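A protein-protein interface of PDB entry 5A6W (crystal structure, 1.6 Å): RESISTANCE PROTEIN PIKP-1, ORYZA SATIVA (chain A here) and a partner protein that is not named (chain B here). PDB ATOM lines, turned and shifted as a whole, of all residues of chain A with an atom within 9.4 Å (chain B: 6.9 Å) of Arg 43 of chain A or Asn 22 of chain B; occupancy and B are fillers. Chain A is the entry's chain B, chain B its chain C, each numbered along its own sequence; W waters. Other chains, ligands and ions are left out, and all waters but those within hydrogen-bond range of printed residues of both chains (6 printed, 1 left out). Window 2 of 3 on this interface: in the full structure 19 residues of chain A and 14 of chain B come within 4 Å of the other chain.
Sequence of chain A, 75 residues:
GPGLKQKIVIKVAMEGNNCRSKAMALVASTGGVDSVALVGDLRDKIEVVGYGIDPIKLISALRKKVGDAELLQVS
The side-chain carboxylate of Asp 46 of chain B sits at hydrogen-bond distance from the backbone NH of Asp 41 of chain A, at 2.7 Å.
The backbone carbonyl oxygen of Gly 40 of chain A sits at hydrogen-bond distance from the side-chain amide nitrogen of Asn 22 of chain B, 3.0 Å away.
The side-chain carboxylate (OD2) of Asp 46 of chain B is in salt-bridge range of the side-chain amino group (NZ) of Lys 45 of chain A, 2.6 Å away.
The guanidinium group (NH2) of Arg 19 of chain B lies within salt-bridge range of the side-chain carboxylate (OD2) of Asp 41 of chain A (3.8 Å).
OD1 of Asp 41 of chain A is in salt-bridge range of NH2 of Arg 44 of chain B.
The backbone carbonyl oxygen (O) of Arg 43 of chain A is in hydrogen-bond range of the guanidinium group (NH1) of Arg 20 of chain A, 2.8 Å away.
O of Val 39 of chain A lies within hydrogen-bond range of N of Asp 44 of chain A, at 3.5 Å.
The guanidinium group of Arg 43 of chain A sits at hydrogen-bond distance from the backbone carbonyl oxygen of Asp 41 of chain A (3.2 Å).
The backbone carbonyl oxygen (O) of Ala 37 of chain A lies within hydrogen-bond range of the backbone NH (N) of Glu 47 of chain A, at 2.8 Å.
The backbone NH (N) of Val 39 of chain A sits at hydrogen-bond distance from the backbone carbonyl oxygen (O) of Lys 45 of chain A, 2.8 Å away.
The backbone carbonyl oxygen of Arg 19 of chain B is in hydrogen-bond range of the guanidinium group of Arg 44 of chain B (2.9 Å).
Among the printed residues, merely in contact across the chains: Arg 43 of chain A with Asn 22 of chain B (3.4 Å), Val 39 of chain A with Asn 22 of chain B (3.4 Å), Gly 40 of chain A with Asp 46 of chain B (3.5 Å), Ala 37 of chain A with Phe 24 of chain B (3.5 Å) and Glu 47 of chain A with Phe 24 of chain B (3.8 Å).
Of the printed residues of chain B, Arg 43 of chain A touches Asn 22.
Of the printed residues of chain A, Asn 22 of chain B touches Val 39, Gly 40 and Arg 43.
Of the printed residues of chain B, Glu 47 of chain A touches Phe 24.
Of the printed residues of chain A, Phe 24 of chain B touches Ala 37 and Glu 47.
The nearest printed residue of chain B that does not touch Asp 41 of chain A is Ala 47 of chain B (4.1 Å).
Of the 11 printed residues of chain B, 5 touch a printed residue of chain A.
Printed residues of chain B that touch a printed residue of chain A: Arg 19, Asn 22, Phe 24, Arg 44 and Asp 46.
Hydrophobic or aromatic side chains of chain B that line the printed part of chain A: Phe 24.
Among the printed residues, 10 pairs touch across the chains.
Among the printed residues, Asp or Glu carboxylates within 4 Å of a Lys or Arg side-chain nitrogen of the other chain: Asp 41 of chain A with Arg 19 of chain B, Asp 41 of chain A with Arg 44 of chain B and Lys 45 of chain A with Asp 46 of chain B.
Water W2 bridges OD2 of Asp 41 of chain A (2.6 Å) and O of Arg 44 of chain B (3.3 Å).
Water W5 bridges the backbone carbonyl oxygen (O) of Leu 38 of chain A and the side-chain amide nitrogen (ND2) of Asn 22 of chain B.
Water W1 lies within hydrogen-bond range of OD1 of Asp 44 of chain A (2.7 Å), N of Leu 42 of chain A (2.9 Å), OD2 of Asp 46 of chain B (3.0 Å) and N of Asp 41 of chain A (3.2 Å).
Water W4 bridges the side-chain carboxylate of Glu 47 of chain A (2.7 Å) and the side-chain hydroxyl of Thr 49 of chain B (2.7 Å).
Water W6 lies within hydrogen-bond range of the side-chain carboxylate (OE1) of Glu 47 of chain A (2.8 Å), the backbone NH (N) of Phe 24 of chain B (2.9 Å) and the side-chain hydroxyl (OG1) of Thr 49 of chain B (3.4 Å).
Water W3 lies within hydrogen-bond range of the side-chain carboxylate (OD1) of Asp 41 of chain A (3.1 Å) and the guanidinium group (NE) of Arg 19 of chain B (3.4 Å).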
ATOM      1  N   VAL A   9      26.701  -4.299 -36.575  1.00  0.00           N
ATOM      2  CA  VAL A   9      26.164  -3.236 -35.741  1.00  0.00           C
ATOM      3  C   VAL A   9      24.852  -2.776 -36.337  1.00  0.00           C
ATOM      4  O   VAL A   9      24.776  -2.503 -37.553  1.00  0.00           O
ATOM      5  CB  VAL A   9      27.127  -2.058 -35.646  1.00  0.00           C
ATOM      6  CG1 VAL A   9      26.553  -0.960 -34.754  1.00  0.00           C
ATOM      7  CG2 VAL A   9      28.496  -2.562 -35.142  1.00  0.00           C
ATOM      8  N   ILE A  10      23.816  -2.717 -35.509  1.00  0.00           N
ATOM      9  CA  ILE A  10      22.463  -2.339 -35.917  1.00  0.00           C
ATOM     10  C   ILE A  10      21.976  -1.175 -35.041  1.00  0.00           C
ATOM     11  O   ILE A  10      22.112  -1.190 -33.813  1.00  0.00           O
ATOM     12  CB  ILE A  10      21.501  -3.535 -35.788  1.00  0.00           C
ATOM     13  CG1 ILE A  10      21.906  -4.653 -36.762  1.00  0.00           C
ATOM     14  CG2 ILE A  10      20.069  -3.102 -35.992  1.00  0.00           C
ATOM     15  CD1 ILE A  10      21.235  -5.991 -36.420  1.00  0.00           C
ATOM     16  N   LYS A  11      21.429  -0.166 -35.690  1.00  0.00           N
ATOM     17  CA  LYS A  11      20.752   0.904 -34.961  1.00  0.00           C
ATOM     18  C   LYS A  11      19.297   0.556 -34.815  1.00  0.00           C
ATOM     19  O   LYS A  11      18.616   0.177 -35.767  1.00  0.00           O
ATOM     20  CB  LYS A  11      20.895   2.249 -35.680  1.00  0.00           C
ATOM     21  CG  LYS A  11      20.307   3.425 -34.940  1.00  0.00           C
ATOM     22  CD  LYS A  11      20.605   4.696 -35.690  1.00  0.00           C
ATOM     23  CE  LYS A  11      19.702   5.823 -35.219  1.00  0.00           C
ATOM     24  NZ  LYS A  11      20.014   7.062 -35.961  1.00  0.00           N
ATOM     25  N   VAL A  12      18.781   0.686 -33.606  1.00  0.00           N
ATOM     26  CA  VAL A  12      17.397   0.371 -33.413  1.00  0.00           C
ATOM     27  C   VAL A  12      16.727   1.589 -32.799  1.00  0.00           C
ATOM     28  O   VAL A  12      17.310   2.259 -31.955  1.00  0.00           O
ATOM     29  CB  VAL A  12      17.180  -0.870 -32.516  1.00  0.00           C
ATOM     30  CG1 VAL A  12      15.715  -1.257 -32.550  1.00  0.00           C
ATOM     31  CG2 VAL A  12      18.004  -2.053 -32.985  1.00  0.00           C
ATOM     32  N   ALA A  13      15.521   1.883 -33.275  1.00  0.00           N
ATOM     33  CA  ALA A  13      14.637   2.857 -32.606  1.00  0.00           C
ATOM     34  C   ALA A  13      14.165   2.236 -31.293  1.00  0.00           C
ATOM     35  O   ALA A  13      13.419   1.261 -31.314  1.00  0.00           O
ATOM     36  CB  ALA A  13      13.451   3.179 -33.497  1.00  0.00           C
ATOM     37  N   MET A  14      14.597   2.795 -30.161  1.00  0.00           N
ATOM     38  CA  MET A  14      14.344   2.202 -28.836  1.00  0.00           C
ATOM     39  C   MET A  14      13.889   3.252 -27.829  1.00  0.00           C
ATOM     40  O   MET A  14      14.708   4.039 -27.356  1.00  0.00           O
ATOM     41  CB  MET A  14      15.618   1.530 -28.289  1.00  0.00           C
ATOM     42  CG  MET A  14      16.017   0.257 -29.012  1.00  0.00           C
ATOM     43  SD  MET A  14      17.607  -0.472 -28.528  1.00  0.00           S
ATOM     44  CE  MET A  14      18.782   0.819 -28.938  1.00  0.00           C
ATOM     45  N   GLU A  15      12.591   3.267 -27.512  1.00  0.00           N
ATOM     46  CA  GLU A  15      12.037   4.136 -26.464  1.00  0.00           C
ATOM     47  C   GLU A  15      10.960   3.392 -25.680  1.00  0.00           C
ATOM     48  O   GLU A  15      10.659   3.742 -24.537  1.00  0.00           O
ATOM     49  CB  GLU A  15      11.444   5.419 -27.059  1.00  0.00           C
ATOM     50  CG  GLU A  15      12.404   6.206 -27.945  1.00  0.00           C
ATOM     51  CD  GLU A  15      12.391   5.744 -29.397  1.00  0.00           C
ATOM     52  OE1 GLU A  15      11.294   5.688 -29.992  1.00  0.00           O
ATOM     53  OE2 GLU A  15      13.474   5.439 -29.949  1.00  0.00           O
ATOM     54  N   ARG A  20      14.291  -1.078 -25.654  1.00  0.00           N
ATOM     55  CA  ARG A  20      15.709  -1.318 -25.451  1.00  0.00           C
ATOM     56  C   ARG A  20      15.961  -2.747 -24.994  1.00  0.00           C
ATOM     57  O   ARG A  20      16.764  -3.461 -25.609  1.00  0.00           O
ATOM     58  CB  ARG A  20      16.272  -0.336 -24.422  1.00  0.00           C
ATOM     59  CG  ARG A  20      17.775  -0.444 -24.194  1.00  0.00           C
ATOM     60  CD  ARG A  20      18.294   0.750 -23.399  1.00  0.00           C
ATOM     61  NE  ARG A  20      18.182   1.985 -24.181  1.00  0.00           N
ATOM     62  CZ  ARG A  20      19.191   2.646 -24.749  1.00  0.00           C
ATOM     63  NH1 ARG A  20      20.452   2.246 -24.618  1.00  0.00           N
ATOM     64  NH2 ARG A  20      18.931   3.748 -25.440  1.00  0.00           N
ATOM     65  N   MET A  24      17.533  -6.008 -27.245  1.00  0.00           N
ATOM     66  CA  MET A  24      18.665  -6.767 -26.735  1.00  0.00           C
ATOM     67  C   MET A  24      18.292  -8.213 -26.562  1.00  0.00           C
ATOM     68  O   MET A  24      19.058  -9.110 -26.916  1.00  0.00           O
ATOM     69  CB  MET A  24      19.102  -6.204 -25.381  1.00  0.00           C
ATOM     70  CG  MET A  24      19.765  -4.838 -25.482  1.00  0.00           C
ATOM     71  SD  MET A  24      21.400  -4.960 -26.216  1.00  0.00           S
ATOM     72  CE  MET A  24      22.396  -5.620 -24.872  1.00  0.00           C
ATOM     73  N   ALA A  37      26.138  -5.994 -27.264  1.00  0.00           N
ATOM     74  CA  ALA A  37      26.394  -4.817 -26.447  1.00  0.00           C
ATOM     75  C   ALA A  37      25.731  -3.585 -27.043  1.00  0.00           C
ATOM     76  O   ALA A  37      25.748  -3.371 -28.243  1.00  0.00           O
ATOM     77  CB  ALA A  37      27.896  -4.535 -26.347  1.00  0.00           C
ATOM     78  N   LEU A  38      25.252  -2.715 -26.150  1.00  0.00           N
ATOM     79  CA  LEU A  38      24.767  -1.371 -26.519  1.00  0.00           C
ATOM     80  C   LEU A  38      25.918  -0.439 -26.514  1.00  0.00           C
ATOM     81  O   LEU A  38      26.591  -0.298 -25.500  1.00  0.00           O
ATOM     82  CB  LEU A  38      23.724  -0.865 -25.532  1.00  0.00           C
ATOM     83  CG  LEU A  38      22.362  -1.447 -25.786  1.00  0.00           C
ATOM     84  CD1 LEU A  38      21.558  -1.424 -24.494  1.00  0.00           C
ATOM     85  CD2 LEU A  38      21.679  -0.634 -26.895  1.00  0.00           C
ATOM     86  N   VAL A  39      26.145   0.207 -27.648  1.00  0.00           N
ATOM     87  CA  VAL A  39      27.327   1.034 -27.857  1.00  0.00           C
ATOM     88  C   VAL A  39      26.920   2.318 -28.590  1.00  0.00           C
ATOM     89  O   VAL A  39      25.751   2.517 -28.976  1.00  0.00           O
ATOM     90  CB  VAL A  39      28.387   0.288 -28.687  1.00  0.00           C
ATOM     91  CG1 VAL A  39      28.878  -0.931 -27.917  1.00  0.00           C
ATOM     92  CG2 VAL A  39      27.858  -0.080 -30.068  1.00  0.00           C
ATOM     93  N   GLY A  40      27.919   3.155 -28.833  1.00  0.00           N
ATOM     94  CA  GLY A  40      27.750   4.372 -29.614  1.00  0.00           C
ATOM     95  C   GLY A  40      27.613   5.603 -28.756  1.00  0.00           C
ATOM     96  O   GLY A  40      27.276   5.533 -27.574  1.00  0.00           O
ATOM     97  N   ASP A  41      27.820   6.783 -29.357  1.00  0.00           N
ATOM     98  CA  ASP A  41      27.798   7.986 -28.571  1.00  0.00           C
ATOM     99  C   ASP A  41      26.392   8.226 -27.970  1.00  0.00           C
ATOM    100  O   ASP A  41      26.265   8.837 -26.898  1.00  0.00           O
ATOM    101  CB  ASP A  41      28.165   9.183 -29.460  1.00  0.00           C
ATOM    102  CG  ASP A  41      29.657   9.295 -29.813  1.00  0.00           C
ATOM    103  OD1 ASP A  41      30.501   8.556 -29.213  1.00  0.00           O
ATOM    104  OD2 ASP A  41      29.957  10.151 -30.708  1.00  0.00           O
ATOM    105  N   LEU A  42      25.350   7.774 -28.672  1.00  0.00           N
ATOM    106  CA  LEU A  42      23.966   7.889 -28.162  1.00  0.00           C
ATOM    107  C   LEU A  42      23.384   6.588 -27.574  1.00  0.00           C
ATOM    108  O   LEU A  42      22.186   6.522 -27.272  1.00  0.00           O
ATOM    109  CB  LEU A  42      23.043   8.442 -29.255  1.00  0.00           C
ATOM    110  CG  LEU A  42      23.303   9.905 -29.636  1.00  0.00           C
ATOM    111  CD1 LEU A  42      22.359  10.281 -30.767  1.00  0.00           C
ATOM    112  CD2 LEU A  42      23.081  10.844 -28.469  1.00  0.00           C
ATOM    113  N   ARG A  43      24.232   5.586 -27.358  1.00  0.00           N
ATOM    114  CA  ARG A  43      23.780   4.336 -26.765  1.00  0.00           C
ATOM    115  C   ARG A  43      22.530   3.837 -27.469  1.00  0.00           C
ATOM    116  O   ARG A  43      21.540   3.479 -26.827  1.00  0.00           O
ATOM    117  CB  ARG A  43      23.531   4.532 -25.265  1.00  0.00           C
ATOM    118  CG  ARG A  43      24.821   4.713 -24.505  1.00  0.00           C
ATOM    119  CD  ARG A  43      25.118   6.144 -24.086  1.00  0.00           C
ATOM    120  NE  ARG A  43      26.221   6.110 -23.132  1.00  0.00           N
ATOM    121  CZ  ARG A  43      27.422   6.620 -23.363  1.00  0.00           C
ATOM    122  NH1 ARG A  43      27.660   7.261 -24.498  1.00  0.00           N
ATOM    123  NH2 ARG A  43      28.375   6.507 -22.443  1.00  0.00           N
ATOM    124  N   ASP A  44      22.570   3.854 -28.797  1.00  0.00           N
ATOM    125  CA  ASP A  44      21.448   3.455 -29.621  1.00  0.00           C
ATOM    126  C   ASP A  44      21.800   2.414 -30.652  1.00  0.00           C
ATOM    127  O   ASP A  44      21.016   2.153 -31.573  1.00  0.00           O
ATOM    128  CB  ASP A  44      20.852   4.672 -30.334  1.00  0.00           C
ATOM    129  CG  ASP A  44      21.859   5.418 -31.210  1.00  0.00           C
ATOM    130  OD1 ASP A  44      23.079   5.131 -31.169  1.00  0.00           O
ATOM    131  OD2 ASP A  44      21.415   6.366 -31.886  1.00  0.00           O
ATOM    132  N   LYS A  45      22.981   1.823 -30.512  1.00  0.00           N
ATOM    133  CA  LYS A  45      23.432   0.858 -31.491  1.00  0.00           C
ATOM    134  C   LYS A  45      23.724  -0.443 -30.776  1.00  0.00           C
ATOM    135  O   LYS A  45      24.274  -0.425 -29.670  1.00  0.00           O
ATOM    136  CB  LYS A  45      24.661   1.407 -32.189  1.00  0.00           C
ATOM    137  CG  LYS A  45      24.272   2.516 -33.155  1.00  0.00           C
ATOM    138  CD  LYS A  45      25.450   3.265 -33.675  1.00  0.00           C
ATOM    139  CE  LYS A  45      24.973   4.505 -34.392  1.00  0.00           C
ATOM    140  NZ  LYS A  45      26.101   5.162 -35.110  1.00  0.00           N
ATOM    141  N   ILE A  46      23.334  -1.545 -31.379  1.00  0.00           N
ATOM    142  CA  ILE A  46      23.614  -2.853 -30.807  1.00  0.00           C
ATOM    143  C   ILE A  46      24.684  -3.531 -31.649  1.00  0.00           C
ATOM    144  O   ILE A  46      24.545  -3.692 -32.870  1.00  0.00           O
ATOM    145  CB  ILE A  46      22.335  -3.701 -30.759  1.00  0.00           C
ATOM    146  CG1 ILE A  46      21.311  -3.002 -29.857  1.00  0.00           C
ATOM    147  CG2 ILE A  46      22.672  -5.119 -30.346  1.00  0.00           C
ATOM    148  CD1 ILE A  46      19.973  -3.725 -29.813  1.00  0.00           C
ATOM    149  N   GLU A  47      25.775  -3.912 -30.997  1.00  0.00           N
ATOM    150  CA  GLU A  47      26.816  -4.633 -31.653  1.00  0.00           C
ATOM    151  C   GLU A  47      26.687  -6.122 -31.284  1.00  0.00           C
ATOM    152  O   GLU A  47      26.601  -6.455 -30.098  1.00  0.00           O
ATOM    153  CB  GLU A  47      28.116  -3.996 -31.214  1.00  0.00           C
ATOM    154  CG  GLU A  47      29.344  -4.450 -31.936  1.00  0.00           C
ATOM    155  CD  GLU A  47      30.521  -3.612 -31.486  1.00  0.00           C
ATOM    156  OE1 GLU A  47      31.071  -3.879 -30.402  1.00  0.00           O
ATOM    157  OE2 GLU A  47      30.837  -2.620 -32.155  1.00  0.00           O
ATOM    158  N   ARG B  19      36.885  12.567 -26.839  1.00  0.00           N
ATOM    159  CA  ARG B  19      36.592  11.584 -25.824  1.00  0.00           C
ATOM    160  C   ARG B  19      36.569  10.185 -26.430  1.00  0.00           C
ATOM    161  O   ARG B  19      36.219  10.001 -27.593  1.00  0.00           O
ATOM    162  CB  ARG B  19      35.277  11.916 -25.141  1.00  0.00           C
ATOM    163  CG  ARG B  19      34.039  11.611 -25.907  1.00  0.00           C
ATOM    164  CD  ARG B  19      32.850  12.341 -25.306  1.00  0.00           C
ATOM    165  NE  ARG B  19      31.598  12.042 -25.962  1.00  0.00           N
ATOM    166  CZ  ARG B  19      31.186  12.606 -27.094  1.00  0.00           C
ATOM    167  NH1 ARG B  19      31.952  13.478 -27.737  1.00  0.00           N
ATOM    168  NH2 ARG B  19      30.012  12.264 -27.601  1.00  0.00           N
ATOM    169  N   ASP B  20      36.984   9.196 -25.650  1.00  0.00           N
ATOM    170  CA  ASP B  20      36.943   7.832 -26.178  1.00  0.00           C
ATOM    171  C   ASP B  20      35.544   7.421 -26.577  1.00  0.00           C
ATOM    172  O   ASP B  20      34.541   7.859 -25.994  1.00  0.00           O
ATOM    173  CB  ASP B  20      37.434   6.858 -25.104  1.00  0.00           C
ATOM    174  CG  ASP B  20      38.902   6.911 -24.866  1.00  0.00           C
ATOM    175  OD1 ASP B  20      39.701   7.623 -25.512  1.00  0.00           O
ATOM    176  OD2 ASP B  20      39.309   6.172 -23.921  1.00  0.00           O
ATOM    177  N   PRO B  21      35.435   6.525 -27.556  1.00  0.00           N
ATOM    178  CA  PRO B  21      34.133   5.968 -27.884  1.00  0.00           C
ATOM    179  C   PRO B  21      33.524   5.197 -26.721  1.00  0.00           C
ATOM    180  O   PRO B  21      34.237   4.805 -25.785  1.00  0.00           O
ATOM    181  CB  PRO B  21      34.449   4.959 -29.017  1.00  0.00           C
ATOM    182  CG  PRO B  21      35.793   5.361 -29.543  1.00  0.00           C
ATOM    183  CD  PRO B  21      36.522   5.963 -28.364  1.00  0.00           C
ATOM    184  N   ASN B  22      32.220   4.977 -26.821  1.00  0.00           N
ATOM    185  CA  ASN B  22      31.504   4.064 -25.944  1.00  0.00           C
ATOM    186  C   ASN B  22      31.537   2.703 -26.631  1.00  0.00           C
ATOM    187  O   ASN B  22      30.767   2.481 -27.581  1.00  0.00           O
ATOM    188  CB  ASN B  22      30.078   4.615 -25.718  1.00  0.00           C
ATOM    189  CG  ASN B  22      29.183   3.668 -24.954  1.00  0.00           C
ATOM    190  OD1 ASN B  22      29.648   2.937 -24.084  1.00  0.00           O
ATOM    191  ND2 ASN B  22      27.914   3.647 -25.296  1.00  0.00           N
ATOM    192  N   PHE B  23      32.399   1.804 -26.131  1.00  0.00           N
ATOM    193  CA  PHE B  23      32.688   0.533 -26.779  1.00  0.00           C
ATOM    194  C   PHE B  23      32.565  -0.656 -25.813  1.00  0.00           C
ATOM    195  O   PHE B  23      32.474  -0.491 -24.583  1.00  0.00           O
ATOM    196  CB  PHE B  23      34.109   0.555 -27.408  1.00  0.00           C
ATOM    197  CG  PHE B  23      35.209   0.636 -26.389  1.00  0.00           C
ATOM    198  CD1 PHE B  23      35.718  -0.487 -25.744  1.00  0.00           C
ATOM    199  CD2 PHE B  23      35.660   1.877 -25.946  1.00  0.00           C
ATOM    200  CE1 PHE B  23      36.672  -0.376 -24.759  1.00  0.00           C
ATOM    201  CE2 PHE B  23      36.623   1.986 -24.972  1.00  0.00           C
ATOM    202  CZ  PHE B  23      37.130   0.866 -24.354  1.00  0.00           C
ATOM    203  N   PHE B  24      32.610  -1.848 -26.389  1.00  0.00           N
ATOM    204  CA  PHE B  24      32.637  -3.072 -25.615  1.00  0.00           C
ATOM    205  C   PHE B  24      33.612  -4.040 -26.275  1.00  0.00           C
ATOM    206  O   PHE B  24      33.427  -4.394 -27.464  1.00  0.00           O
ATOM    207  CB  PHE B  24      31.235  -3.690 -25.539  1.00  0.00           C
ATOM    208  CG  PHE B  24      31.189  -5.009 -24.850  1.00  0.00           C
ATOM    209  CD1 PHE B  24      31.430  -5.103 -23.487  1.00  0.00           C
ATOM    210  CD2 PHE B  24      30.989  -6.183 -25.542  1.00  0.00           C
ATOM    211  CE1 PHE B  24      31.385  -6.298 -22.868  1.00  0.00           C
ATOM    212  CE2 PHE B  24      30.915  -7.404 -24.902  1.00  0.00           C
ATOM    213  CZ  PHE B  24      31.144  -7.469 -23.566  1.00  0.00           C
ATOM    214  N   ARG B  44      31.521  15.583 -34.960  1.00  0.00           N
ATOM    215  CA  ARG B  44      31.493  14.161 -34.603  1.00  0.00           C
ATOM    216  C   ARG B  44      30.063  13.613 -34.621  1.00  0.00           C
ATOM    217  O   ARG B  44      29.142  14.174 -34.016  1.00  0.00           O
ATOM    218  CB  ARG B  44      32.105  13.950 -33.233  1.00  0.00           C
ATOM    219  CG  ARG B  44      32.038  12.509 -32.723  1.00  0.00           C
ATOM    220  CD  ARG B  44      32.856  12.386 -31.469  1.00  0.00           C
ATOM    221  NE  ARG B  44      32.614  11.154 -30.715  1.00  0.00           N
ATOM    222  CZ  ARG B  44      33.412  10.712 -29.733  1.00  0.00           C
ATOM    223  NH1 ARG B  44      34.529  11.359 -29.471  1.00  0.00           N
ATOM    224  NH2 ARG B  44      33.095   9.610 -29.038  1.00  0.00           N
ATOM    225  N   ASP B  46      29.656   9.762 -34.593  1.00  0.00           N
ATOM    226  CA  ASP B  46      29.773   8.599 -33.720  1.00  0.00           C
ATOM    227  C   ASP B  46      31.220   8.149 -33.734  1.00  0.00           C
ATOM    228  O   ASP B  46      32.069   8.724 -34.415  1.00  0.00           O
ATOM    229  CB  ASP B  46      28.863   7.440 -34.125  1.00  0.00           C
ATOM    230  CG  ASP B  46      28.486   6.552 -32.930  1.00  0.00           C
ATOM    231  OD1 ASP B  46      28.996   6.756 -31.797  1.00  0.00           O
ATOM    232  OD2 ASP B  46      27.606   5.731 -33.097  1.00  0.00           O
ATOM    233  N   ALA B  47      31.506   7.089 -32.968  1.00  0.00           N
ATOM    234  CA  ALA B  47      32.860   6.608 -32.808  1.00  0.00           C
ATOM    235  C   ALA B  47      32.783   5.194 -32.314  1.00  0.00           C
ATOM    236  O   ALA B  47      31.785   4.775 -31.726  1.00  0.00           O
ATOM    237  CB  ALA B  47      33.629   7.461 -31.807  1.00  0.00           C
ATOM    238  N   GLY B  48      33.849   4.427 -32.536  1.00  0.00           N
ATOM    239  CA  GLY B  48      33.847   3.044 -32.079  1.00  0.00           C
ATOM    240  C   GLY B  48      35.213   2.444 -32.184  1.00  0.00           C
ATOM    241  O   GLY B  48      36.210   3.171 -32.312  1.00  0.00           O
ATOM    242  N   THR B  49      35.276   1.108 -32.125  1.00  0.00           N
ATOM    243  CA  THR B  49      36.531   0.404 -32.277  1.00  0.00           C
ATOM    244  C   THR B  49      36.591  -0.329 -33.591  1.00  0.00           C
ATOM    245  O   THR B  49      35.580  -0.706 -34.180  1.00  0.00           O
ATOM    246  CB  THR B  49      36.725  -0.639 -31.158  1.00  0.00           C
ATOM    247  OG1 THR B  49      35.609  -1.544 -31.149  1.00  0.00           O
ATOM    248  CG2 THR B  49      36.887   0.046 -29.820  1.00  0.00           C
HETATM  249  O   HOH W   1      25.350   6.581 -31.317  1.00  0.00           O
HETATM  250  O   HOH W   2      28.517  12.191 -31.497  1.00  0.00           O
HETATM  251  O   HOH W   3      30.846   8.705 -26.166  1.00  0.00           O
HETATM  252  O   HOH W   4      33.506  -2.434 -32.628  1.00  0.00           O
HETATM  253  O   HOH W   5      26.152   1.728 -23.816  1.00  0.00           O
HETATM  254  O   HOH W   6      32.850  -2.039 -29.229  1.00  0.00           O
